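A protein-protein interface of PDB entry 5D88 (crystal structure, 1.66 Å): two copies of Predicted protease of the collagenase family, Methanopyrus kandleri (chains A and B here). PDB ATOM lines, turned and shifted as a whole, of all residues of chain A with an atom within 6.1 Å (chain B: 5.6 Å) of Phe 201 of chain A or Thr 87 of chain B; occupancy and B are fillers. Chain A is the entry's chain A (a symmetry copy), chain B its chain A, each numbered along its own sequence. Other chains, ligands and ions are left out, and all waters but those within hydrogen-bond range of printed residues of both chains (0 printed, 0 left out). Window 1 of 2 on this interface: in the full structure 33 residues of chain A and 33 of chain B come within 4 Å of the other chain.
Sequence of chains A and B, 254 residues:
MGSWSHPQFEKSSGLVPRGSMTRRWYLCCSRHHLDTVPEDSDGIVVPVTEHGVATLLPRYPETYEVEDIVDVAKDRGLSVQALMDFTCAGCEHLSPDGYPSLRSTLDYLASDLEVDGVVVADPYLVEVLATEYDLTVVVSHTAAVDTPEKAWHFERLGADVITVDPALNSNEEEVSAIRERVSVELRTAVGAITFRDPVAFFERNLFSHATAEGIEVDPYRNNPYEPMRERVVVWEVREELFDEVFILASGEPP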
ATOM      1  N   THR A  87      -3.443  -5.040  10.016  1.00  0.00           N
ATOM      2  CA  THR A  87      -4.477  -5.835   9.375  1.00  0.00           C
ATOM      3  C   THR A  87      -5.786  -5.815  10.139  1.00  0.00           C
ATOM      4  O   THR A  87      -6.779  -6.393   9.670  1.00  0.00           O
ATOM      5  CB  THR A  87      -3.988  -7.274   9.180  1.00  0.00           C
ATOM      6  OG1 THR A  87      -3.486  -7.814  10.413  1.00  0.00           O
ATOM      7  CG2 THR A  87      -2.898  -7.289   8.110  1.00  0.00           C
ATOM      8  N   PHE A 195       1.825 -15.403   3.608  1.00  0.00           N
ATOM      9  CA  PHE A 195       0.558 -15.782   4.195  1.00  0.00           C
ATOM     10  C   PHE A 195       0.324 -17.286   4.150  1.00  0.00           C
ATOM     11  O   PHE A 195      -0.570 -17.778   4.849  1.00  0.00           O
ATOM     12  CB  PHE A 195      -0.569 -15.025   3.470  1.00  0.00           C
ATOM     13  CG  PHE A 195      -1.798 -14.893   4.267  1.00  0.00           C
ATOM     14  CD1 PHE A 195      -1.943 -13.840   5.159  1.00  0.00           C
ATOM     15  CD2 PHE A 195      -2.825 -15.808   4.126  1.00  0.00           C
ATOM     16  CE1 PHE A 195      -3.092 -13.684   5.892  1.00  0.00           C
ATOM     17  CE2 PHE A 195      -3.983 -15.681   4.885  1.00  0.00           C
ATOM     18  CZ  PHE A 195      -4.112 -14.609   5.773  1.00  0.00           C
ATOM     19  N   ASP A 197       2.255 -19.216   5.556  1.00  0.00           N
ATOM     20  CA  ASP A 197       2.628 -19.587   6.911  1.00  0.00           C
ATOM     21  C   ASP A 197       1.365 -19.894   7.709  1.00  0.00           C
ATOM     22  O   ASP A 197       0.412 -19.106   7.694  1.00  0.00           O
ATOM     23  CB  ASP A 197       3.427 -18.430   7.549  1.00  0.00           C
ATOM     24  CG  ASP A 197       3.824 -18.672   8.989  1.00  0.00           C
ATOM     25  OD1 ASP A 197       2.965 -18.588   9.880  1.00  0.00           O
ATOM     26  OD2 ASP A 197       5.029 -18.890   9.240  1.00  0.00           O
ATOM     27  N   PRO A 198       1.331 -20.983   8.455  1.00  0.00           N
ATOM     28  CA  PRO A 198       0.050 -21.396   9.058  1.00  0.00           C
ATOM     29  C   PRO A 198      -0.581 -20.393  10.036  1.00  0.00           C
ATOM     30  O   PRO A 198      -1.807 -20.361  10.161  1.00  0.00           O
ATOM     31  CB  PRO A 198       0.416 -22.703   9.765  1.00  0.00           C
ATOM     32  CG  PRO A 198       1.929 -22.595  10.018  1.00  0.00           C
ATOM     33  CD  PRO A 198       2.425 -21.932   8.757  1.00  0.00           C
ATOM     34  N   VAL A 199       0.195 -19.584  10.751  1.00  0.00           N
ATOM     35  CA  VAL A 199      -0.369 -18.741  11.801  1.00  0.00           C
ATOM     36  C   VAL A 199      -0.060 -17.260  11.599  1.00  0.00           C
ATOM     37  O   VAL A 199      -0.470 -16.440  12.422  1.00  0.00           O
ATOM     38  CB  VAL A 199       0.064 -19.211  13.205  1.00  0.00           C
ATOM     39  CG1 VAL A 199      -0.155 -20.711  13.361  1.00  0.00           C
ATOM     40  CG2 VAL A 199       1.448 -18.879  13.478  1.00  0.00           C
ATOM     41  N   ALA A 200       0.595 -16.882  10.493  1.00  0.00           N
ATOM     42  CA  ALA A 200       1.014 -15.491  10.320  1.00  0.00           C
ATOM     43  C   ALA A 200      -0.165 -14.525  10.390  1.00  0.00           C
ATOM     44  O   ALA A 200      -0.038 -13.441  10.962  1.00  0.00           O
ATOM     45  CB  ALA A 200       1.767 -15.328   9.000  1.00  0.00           C
ATOM     46  N   PHE A 201      -1.291 -14.876   9.757  1.00  0.00           N
ATOM     47  CA  PHE A 201      -2.528 -14.085   9.795  1.00  0.00           C
ATOM     48  C   PHE A 201      -2.856 -13.634  11.222  1.00  0.00           C
ATOM     49  O   PHE A 201      -3.081 -12.445  11.498  1.00  0.00           O
ATOM     50  CB  PHE A 201      -3.568 -15.026   9.153  1.00  0.00           C
ATOM     51  CG  PHE A 201      -5.009 -14.704   9.301  1.00  0.00           C
ATOM     52  CD1 PHE A 201      -5.507 -13.447   9.464  1.00  0.00           C
ATOM     53  CD2 PHE A 201      -5.908 -15.754   9.083  1.00  0.00           C
ATOM     54  CE1 PHE A 201      -6.915 -13.248   9.532  1.00  0.00           C
ATOM     55  CE2 PHE A 201      -7.250 -15.588   9.141  1.00  0.00           C
ATOM     56  CZ  PHE A 201      -7.773 -14.325   9.360  1.00  0.00           C
ATOM     57  N   PHE A 202      -2.830 -14.583  12.155  1.00  0.00           N
ATOM     58  CA  PHE A 202      -3.232 -14.314  13.520  1.00  0.00           C
ATOM     59  C   PHE A 202      -2.161 -13.520  14.257  1.00  0.00           C
ATOM     60  O   PHE A 202      -2.476 -12.630  15.054  1.00  0.00           O
ATOM     61  CB  PHE A 202      -3.520 -15.643  14.222  1.00  0.00           C
ATOM     62  CG  PHE A 202      -4.571 -16.456  13.513  1.00  0.00           C
ATOM     63  CD1 PHE A 202      -5.916 -16.185  13.722  1.00  0.00           C
ATOM     64  CD2 PHE A 202      -4.217 -17.439  12.602  1.00  0.00           C
ATOM     65  CE1 PHE A 202      -6.892 -16.896  13.059  1.00  0.00           C
ATOM     66  CE2 PHE A 202      -5.193 -18.160  11.912  1.00  0.00           C
ATOM     67  CZ  PHE A 202      -6.533 -17.889  12.143  1.00  0.00           C
ATOM     68  N   GLU A 203      -0.894 -13.841  13.999  1.00  0.00           N
ATOM     69  CA  GLU A 203       0.195 -13.158  14.681  1.00  0.00           C
ATOM     70  C   GLU A 203       0.307 -11.711  14.224  1.00  0.00           C
ATOM     71  O   GLU A 203       0.567 -10.819  15.040  1.00  0.00           O
ATOM     72  CB  GLU A 203       1.495 -13.915  14.462  1.00  0.00           C
ATOM     73  CG  GLU A 203       2.650 -13.374  15.285  1.00  0.00           C
ATOM     74  CD  GLU A 203       3.893 -14.223  15.174  1.00  0.00           C
ATOM     75  OE1 GLU A 203       4.071 -14.903  14.146  1.00  0.00           O
ATOM     76  OE2 GLU A 203       4.699 -14.197  16.124  1.00  0.00           O
ATOM     77  N   ARG A 204       0.084 -11.453  12.935  1.00  0.00           N
ATOM     78  CA  ARG A 204       0.090 -10.080  12.449  1.00  0.00           C
ATOM     79  C   ARG A 204      -1.099  -9.285  12.966  1.00  0.00           C
ATOM     80  O   ARG A 204      -0.962  -8.090  13.236  1.00  0.00           O
ATOM     81  CB  ARG A 204       0.117 -10.068  10.932  1.00  0.00           C
ATOM     82  CG  ARG A 204       1.401 -10.582  10.355  1.00  0.00           C
ATOM     83  CD  ARG A 204       1.317 -10.352   8.913  1.00  0.00           C
ATOM     84  NE  ARG A 204       2.532 -10.677   8.209  1.00  0.00           N
ATOM     85  CZ  ARG A 204       2.545 -11.295   7.040  1.00  0.00           C
ATOM     86  NH1 ARG A 204       1.408 -11.679   6.450  1.00  0.00           N
ATOM     87  NH2 ARG A 204       3.694 -11.520   6.451  1.00  0.00           N
ATOM     88  N   ASN A 205      -2.259  -9.928  13.141  1.00  0.00           N
ATOM     89  CA  ASN A 205      -3.372  -9.260  13.814  1.00  0.00           C
ATOM     90  C   ASN A 205      -2.961  -8.845  15.220  1.00  0.00           C
ATOM     91  O   ASN A 205      -3.268  -7.733  15.668  1.00  0.00           O
ATOM     92  CB  ASN A 205      -4.593 -10.186  13.882  1.00  0.00           C
ATOM     93  CG  ASN A 205      -5.379 -10.276  12.570  1.00  0.00           C
ATOM     94  OD1 ASN A 205      -5.225  -9.472  11.642  1.00  0.00           O
ATOM     95  ND2 ASN A 205      -6.289 -11.250  12.527  1.00  0.00           N
ATOM     96  N   LEU A 206      -2.281  -9.739  15.940  1.00  0.00           N
ATOM     97  CA  LEU A 206      -1.834  -9.442  17.297  1.00  0.00           C
ATOM     98  C   LEU A 206      -0.891  -8.244  17.314  1.00  0.00           C
ATOM     99  O   LEU A 206      -1.063  -7.318  18.108  1.00  0.00           O
ATOM    100  CB  LEU A 206      -1.145 -10.662  17.907  1.00  0.00           C
ATOM    101  CG  LEU A 206      -0.610 -10.485  19.338  1.00  0.00           C
ATOM    102  CD1 LEU A 206      -1.732 -10.276  20.338  1.00  0.00           C
ATOM    103  CD2 LEU A 206       0.280 -11.694  19.705  1.00  0.00           C
ATOM    104  N   ALA B  54     -16.378 -14.516  13.716  1.00  0.00           N
ATOM    105  CA  ALA B  54     -15.908 -13.941  12.456  1.00  0.00           C
ATOM    106  C   ALA B  54     -16.818 -14.251  11.278  1.00  0.00           C
ATOM    107  O   ALA B  54     -16.842 -13.498  10.297  1.00  0.00           O
ATOM    108  CB  ALA B  54     -14.503 -14.453  12.138  1.00  0.00           C
ATOM    109  N   ASP B  85     -15.532 -18.299  16.283  1.00  0.00           N
ATOM    110  CA  ASP B  85     -14.454 -18.373  15.306  1.00  0.00           C
ATOM    111  C   ASP B  85     -13.858 -17.016  14.974  1.00  0.00           C
ATOM    112  O   ASP B  85     -13.382 -16.812  13.860  1.00  0.00           O
ATOM    113  CB  ASP B  85     -14.906 -19.087  14.035  1.00  0.00           C
ATOM    114  CG  ASP B  85     -15.963 -18.340  13.250  1.00  0.00           C
ATOM    115  OD1 ASP B  85     -16.572 -17.395  13.745  1.00  0.00           O
ATOM    116  OD2 ASP B  85     -16.187 -18.732  12.095  1.00  0.00           O
ATOM    117  N   PHE B  86     -13.813 -16.114  15.946  1.00  0.00           N
ATOM    118  CA  PHE B  86     -13.102 -14.860  15.770  1.00  0.00           C
ATOM    119  C   PHE B  86     -11.704 -15.079  15.207  1.00  0.00           C
ATOM    120  O   PHE B  86     -11.006 -16.037  15.565  1.00  0.00           O
ATOM    121  CB  PHE B  86     -13.014 -14.083  17.093  1.00  0.00           C
ATOM    122  CG  PHE B  86     -12.288 -14.792  18.198  1.00  0.00           C
ATOM    123  CD1 PHE B  86     -10.908 -14.727  18.283  1.00  0.00           C
ATOM    124  CD2 PHE B  86     -12.997 -15.479  19.173  1.00  0.00           C
ATOM    125  CE1 PHE B  86     -10.247 -15.333  19.302  1.00  0.00           C
ATOM    126  CE2 PHE B  86     -12.343 -16.095  20.219  1.00  0.00           C
ATOM    127  CZ  PHE B  86     -10.960 -16.030  20.283  1.00  0.00           C
ATOM    128  N   THR B  87     -11.287 -14.161  14.332  1.00  0.00           N
ATOM    129  CA  THR B  87      -9.949 -14.198  13.766  1.00  0.00           C
ATOM    130  C   THR B  87      -9.002 -13.226  14.441  1.00  0.00           C
ATOM    131  O   THR B  87      -7.807 -13.202  14.106  1.00  0.00           O
ATOM    132  CB  THR B  87     -10.009 -13.934  12.257  1.00  0.00           C
ATOM    133  OG1 THR B  87     -10.751 -12.736  11.979  1.00  0.00           O
ATOM    134  CG2 THR B  87     -10.657 -15.132  11.567  1.00  0.00           C
ATOM    135  N   CYS B  88      -9.508 -12.433  15.387  1.00  0.00           N
ATOM    136  CA  CYS B  88      -8.709 -11.482  16.144  1.00  0.00           C
ATOM    137  C   CYS B  88      -9.387 -11.243  17.483  1.00  0.00           C
ATOM    138  O   CYS B  88     -10.607 -11.077  17.538  1.00  0.00           O
ATOM    139  CB  CYS B  88      -8.541 -10.149  15.402  1.00  0.00           C
ATOM    140  SG  CYS B  88      -7.314  -9.071  16.183  1.00  0.00           S
ATOM    141  N   ALA B  89      -8.592 -11.274  18.555  1.00  0.00           N
ATOM    142  CA  ALA B  89      -9.046 -10.906  19.891  1.00  0.00           C
ATOM    143  C   ALA B  89      -8.282  -9.697  20.423  1.00  0.00           C
ATOM    144  O   ALA B  89      -8.230  -9.471  21.642  1.00  0.00           O
ATOM    145  CB  ALA B  89      -8.907 -12.097  20.833  1.00  0.00           C
ATOM    146  N   ALA B 121     -11.243 -20.394  15.019  1.00  0.00           N
ATOM    147  CA  ALA B 121     -10.187 -20.095  14.065  1.00  0.00           C
ATOM    148  C   ALA B 121      -8.821 -19.892  14.698  1.00  0.00           C
ATOM    149  O   ALA B 121      -7.811 -20.248  14.099  1.00  0.00           O
ATOM    150  CB  ALA B 121     -10.545 -18.848  13.273  1.00  0.00           C
ATOM    151  N   THR B 142     -13.212 -19.837   8.595  1.00  0.00           N
ATOM    152  CA  THR B 142     -12.628 -18.495   8.652  1.00  0.00           C
ATOM    153  C   THR B 142     -11.127 -18.505   8.924  1.00  0.00           C
ATOM    154  O   THR B 142     -10.486 -17.457   8.799  1.00  0.00           O
ATOM    155  CB  THR B 142     -13.310 -17.650   9.717  1.00  0.00           C
ATOM    156  OG1 THR B 142     -13.124 -18.286  10.990  1.00  0.00           O
ATOM    157  CG2 THR B 142     -14.813 -17.491   9.393  1.00  0.00           C
ATOM    158  N   ALA B 143     -10.556 -19.655   9.286  1.00  0.00           N
ATOM    159  CA  ALA B 143      -9.111 -19.770   9.384  1.00  0.00           C
ATOM    160  C   ALA B 143      -8.434 -19.936   8.022  1.00  0.00           C
ATOM    161  O   ALA B 143      -7.195 -19.921   7.953  1.00  0.00           O
ATOM    162  CB  ALA B 143      -8.746 -20.944  10.285  1.00  0.00           C
ATOM    163  N   ALA B 144      -9.212 -20.140   6.960  1.00  0.00           N
ATOM    164  CA  ALA B 144      -8.706 -20.165   5.580  1.00  0.00           C
ATOM    165  C   ALA B 144      -7.683 -21.282   5.341  1.00  0.00           C
ATOM    166  O   ALA B 144      -6.681 -21.084   4.657  1.00  0.00           O
ATOM    167  CB  ALA B 144      -8.114 -18.815   5.190  1.00  0.00           C
ATOM    168  N   PHE B 195     -11.691 -17.132   1.401  1.00  0.00           N
ATOM    169  CA  PHE B 195     -10.635 -16.175   1.652  1.00  0.00           C
ATOM    170  C   PHE B 195     -10.067 -15.589   0.367  1.00  0.00           C
ATOM    171  O   PHE B 195      -9.364 -14.572   0.428  1.00  0.00           O
ATOM    172  CB  PHE B 195      -9.534 -16.860   2.481  1.00  0.00           C
ATOM    173  CG  PHE B 195      -8.697 -15.919   3.240  1.00  0.00           C
ATOM    174  CD1 PHE B 195      -9.092 -15.490   4.498  1.00  0.00           C
ATOM    175  CD2 PHE B 195      -7.501 -15.464   2.714  1.00  0.00           C
ATOM    176  CE1 PHE B 195      -8.313 -14.633   5.234  1.00  0.00           C
ATOM    177  CE2 PHE B 195      -6.715 -14.573   3.434  1.00  0.00           C
ATOM    178  CZ  PHE B 195      -7.129 -14.157   4.703  1.00  0.00           C
ATOM    179  N   PHE B 201     -10.961 -11.120   4.737  1.00  0.00           N
ATOM    180  CA  PHE B 201     -10.015 -11.109   5.861  1.00  0.00           C
ATOM    181  C   PHE B 201     -10.283  -9.928   6.800  1.00  0.00           C
ATOM    182  O   PHE B 201     -10.434 -10.085   8.022  1.00  0.00           O
ATOM    183  CB  PHE B 201      -8.639 -11.091   5.165  1.00  0.00           C
ATOM    184  CG  PHE B 201      -7.438 -10.756   5.968  1.00  0.00           C
ATOM    185  CD1 PHE B 201      -7.317 -10.978   7.308  1.00  0.00           C
ATOM    186  CD2 PHE B 201      -6.304 -10.348   5.256  1.00  0.00           C
ATOM    187  CE1 PHE B 201      -6.092 -10.676   7.966  1.00  0.00           C
ATOM    188  CE2 PHE B 201      -5.129 -10.057   5.861  1.00  0.00           C
ATOM    189  CZ  PHE B 201      -5.005 -10.225   7.229  1.00  0.00           C
ATOM    190  N   ARG B 204     -14.032  -9.889   8.307  1.00  0.00           N
ATOM    191  CA  ARG B 204     -14.189 -10.851   9.391  1.00  0.00           C
ATOM    192  C   ARG B 204     -13.446 -10.424  10.646  1.00  0.00           C
ATOM    193  O   ARG B 204     -13.929 -10.669  11.753  1.00  0.00           O
ATOM    194  CB  ARG B 204     -13.720 -12.221   8.937  1.00  0.00           C
ATOM    195  CG  ARG B 204     -14.594 -12.831   7.884  1.00  0.00           C
ATOM    196  CD  ARG B 204     -14.098 -14.192   7.685  1.00  0.00           C
ATOM    197  NE  ARG B 204     -14.909 -14.973   6.785  1.00  0.00           N
ATOM    198  CZ  ARG B 204     -14.400 -15.788   5.876  1.00  0.00           C
ATOM    199  NH1 ARG B 204     -13.077 -15.913   5.727  1.00  0.00           N
ATOM    200  NH2 ARG B 204     -15.211 -16.488   5.123  1.00  0.00           N
ATOM    201  N   ASN B 205     -12.293  -9.759  10.502  1.00  0.00           N
ATOM    202  CA  ASN B 205     -11.642  -9.160  11.665  1.00  0.00           C
ATOM    203  C   ASN B 205     -12.572  -8.151  12.326  1.00  0.00           C
ATOM    204  O   ASN B 205     -12.687  -8.106  13.557  1.00  0.00           O
ATOM    205  CB  ASN B 205     -10.335  -8.471  11.255  1.00  0.00           C
ATOM    206  CG  ASN B 205      -9.164  -9.435  11.038  1.00  0.00           C
ATOM    207  OD1 ASN B 205      -9.184 -10.608  11.430  1.00  0.00           O
ATOM    208  ND2 ASN B 205      -8.096  -8.896  10.450  1.00  0.00           N
ATOM    209  N   SER B 208     -15.376  -9.891  14.149  1.00  0.00           N
ATOM    210  CA  SER B 208     -14.827 -10.577  15.314  1.00  0.00           C
ATOM    211  C   SER B 208     -14.856  -9.669  16.526  1.00  0.00           C
ATOM    212  O   SER B 208     -15.103 -10.121  17.650  1.00  0.00           O
ATOM    213  CB  SER B 208     -13.372 -11.018  15.059  1.00  0.00           C
ATOM    214  OG  SER B 208     -13.260 -12.028  14.057  1.00  0.00           O
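O of Thr 87 of chain B lies within hydrogen-bond range of ND2 of Asn 205 of chain A, 2.9 Å away. ND2 of Asn 205 of chain B lies within hydrogen-bond range of O of Thr 87 of chain A, at 2.9 Å. OD1 of Asn 205 of chain A lies within hydrogen-bond range of ND2 of Asn 205 of chain B (3.2 Å).
The side-chain hydroxyl (OG1) of Thr 87 of chain B lies within hydrogen-bond range of the side-chain amide oxygen (OD1) of Asn 205 of chain B (2.7 Å). N of Thr 87 of chain B lies within hydrogen-bond range of OG of Ser 208 of chain B. The backbone carbonyl oxygen (O) of Asp 85 of chain B is in hydrogen-bond range of the side-chain hydroxyl (OG1) of Thr 142 of chain B. The side-chain hydroxyl of Thr 87 of chain A sits at hydrogen-bond distance from the side-chain amide oxygen of Asn 205 of chain A.
Thr 87 of chain A touches Phe 201 of chain B (CB to CZ, 3.7 Å). Phe 195 of chain A touches Phe 195 of chain B (CZ to CZ, 3.2 Å). Phe 201 of chain A touches Thr 87 of chain B (CZ to CB, 3.7 Å). Thr 142 of chain B touches Phe 201 of chain A (O to CE2, 3.8 Å). CE1 of Phe 201 of chain A touches CE1 of Phe 201 of chain B, at 3.1 Å. Phe 201 of chain A touches Asn 205 of chain B (CE1 to OD1, 3.96 Å). Thr 87 of chain B touches Phe 202 of chain A (O to CD1, 3.6 Å). Phe 202 of chain A touches Ala 121 of chain B (CZ to O, 3.3 Å). CB of Asn 205 of chain A touches SG of Cys 88 of chain B (3.7 Å). Asn 205 of chain A touches Phe 201 of chain B (OD1 to CE1, 3.96 Å).
Printed residues of chain B within 4 Å of Phe 201 of chain A: Thr 87 (3.7 Å), Thr 142 (3.8 Å), Phe 201 (3.1 Å) and Asn 205 (3.96 Å). Of chain A, only Phe 201 (3.7 Å), Phe 202 (3.6 Å) and Asn 205 (2.9 Å) come within 4 Å of Thr 87 of chain B. Of the printed residues of chain A, Cys 88 of chain B touches Asn 205. Of the printed residues of chain A, Thr 142 of chain B touches Phe 201. Printed residues of chain A within 4 Å of Phe 195 of chain B: Phe 195. Printed residues of chain A within 4 Å of Asn 205 of chain B: Thr 87, Phe 201 and Asn 205. The nearest residue of chain B that does not touch Phe 201 of chain A is Phe 195 of chain B (4.2 Å). The nearest printed residue of chain A that does not touch Thr 87 of chain B is Leu 206 of chain A (6.8 Å).
Of the 12 printed residues of chain A, 5 touch a printed residue of chain B. Printed residues of chain A that touch a printed residue of chain B: Thr 87, Phe 195, Phe 201, Phe 202 and Asn 205. Of the 15 printed residues of chain B, 7 touch a printed residue of chain A. Hydrophobic or aromatic side chains of chain B within 4 Å of the printed part of chain A: Phe 195 and Phe 201.
Thr 87 of chain A touches Phe 201 of chain B, and with the chains exchanged Phe 201 of chain A touches Thr 87 of chain B. Phe 201 of chain A touches its own counterpart, Phe 201 of chain B. Phe 201 of chain A touches Asn 205 of chain B, and with the chains exchanged Asn 205 of chain A touches Phe 201 of chain B. Asn 205 of chain B touches its own counterpart, Asn 205 of chain A. 5 positions are printed for both chains.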
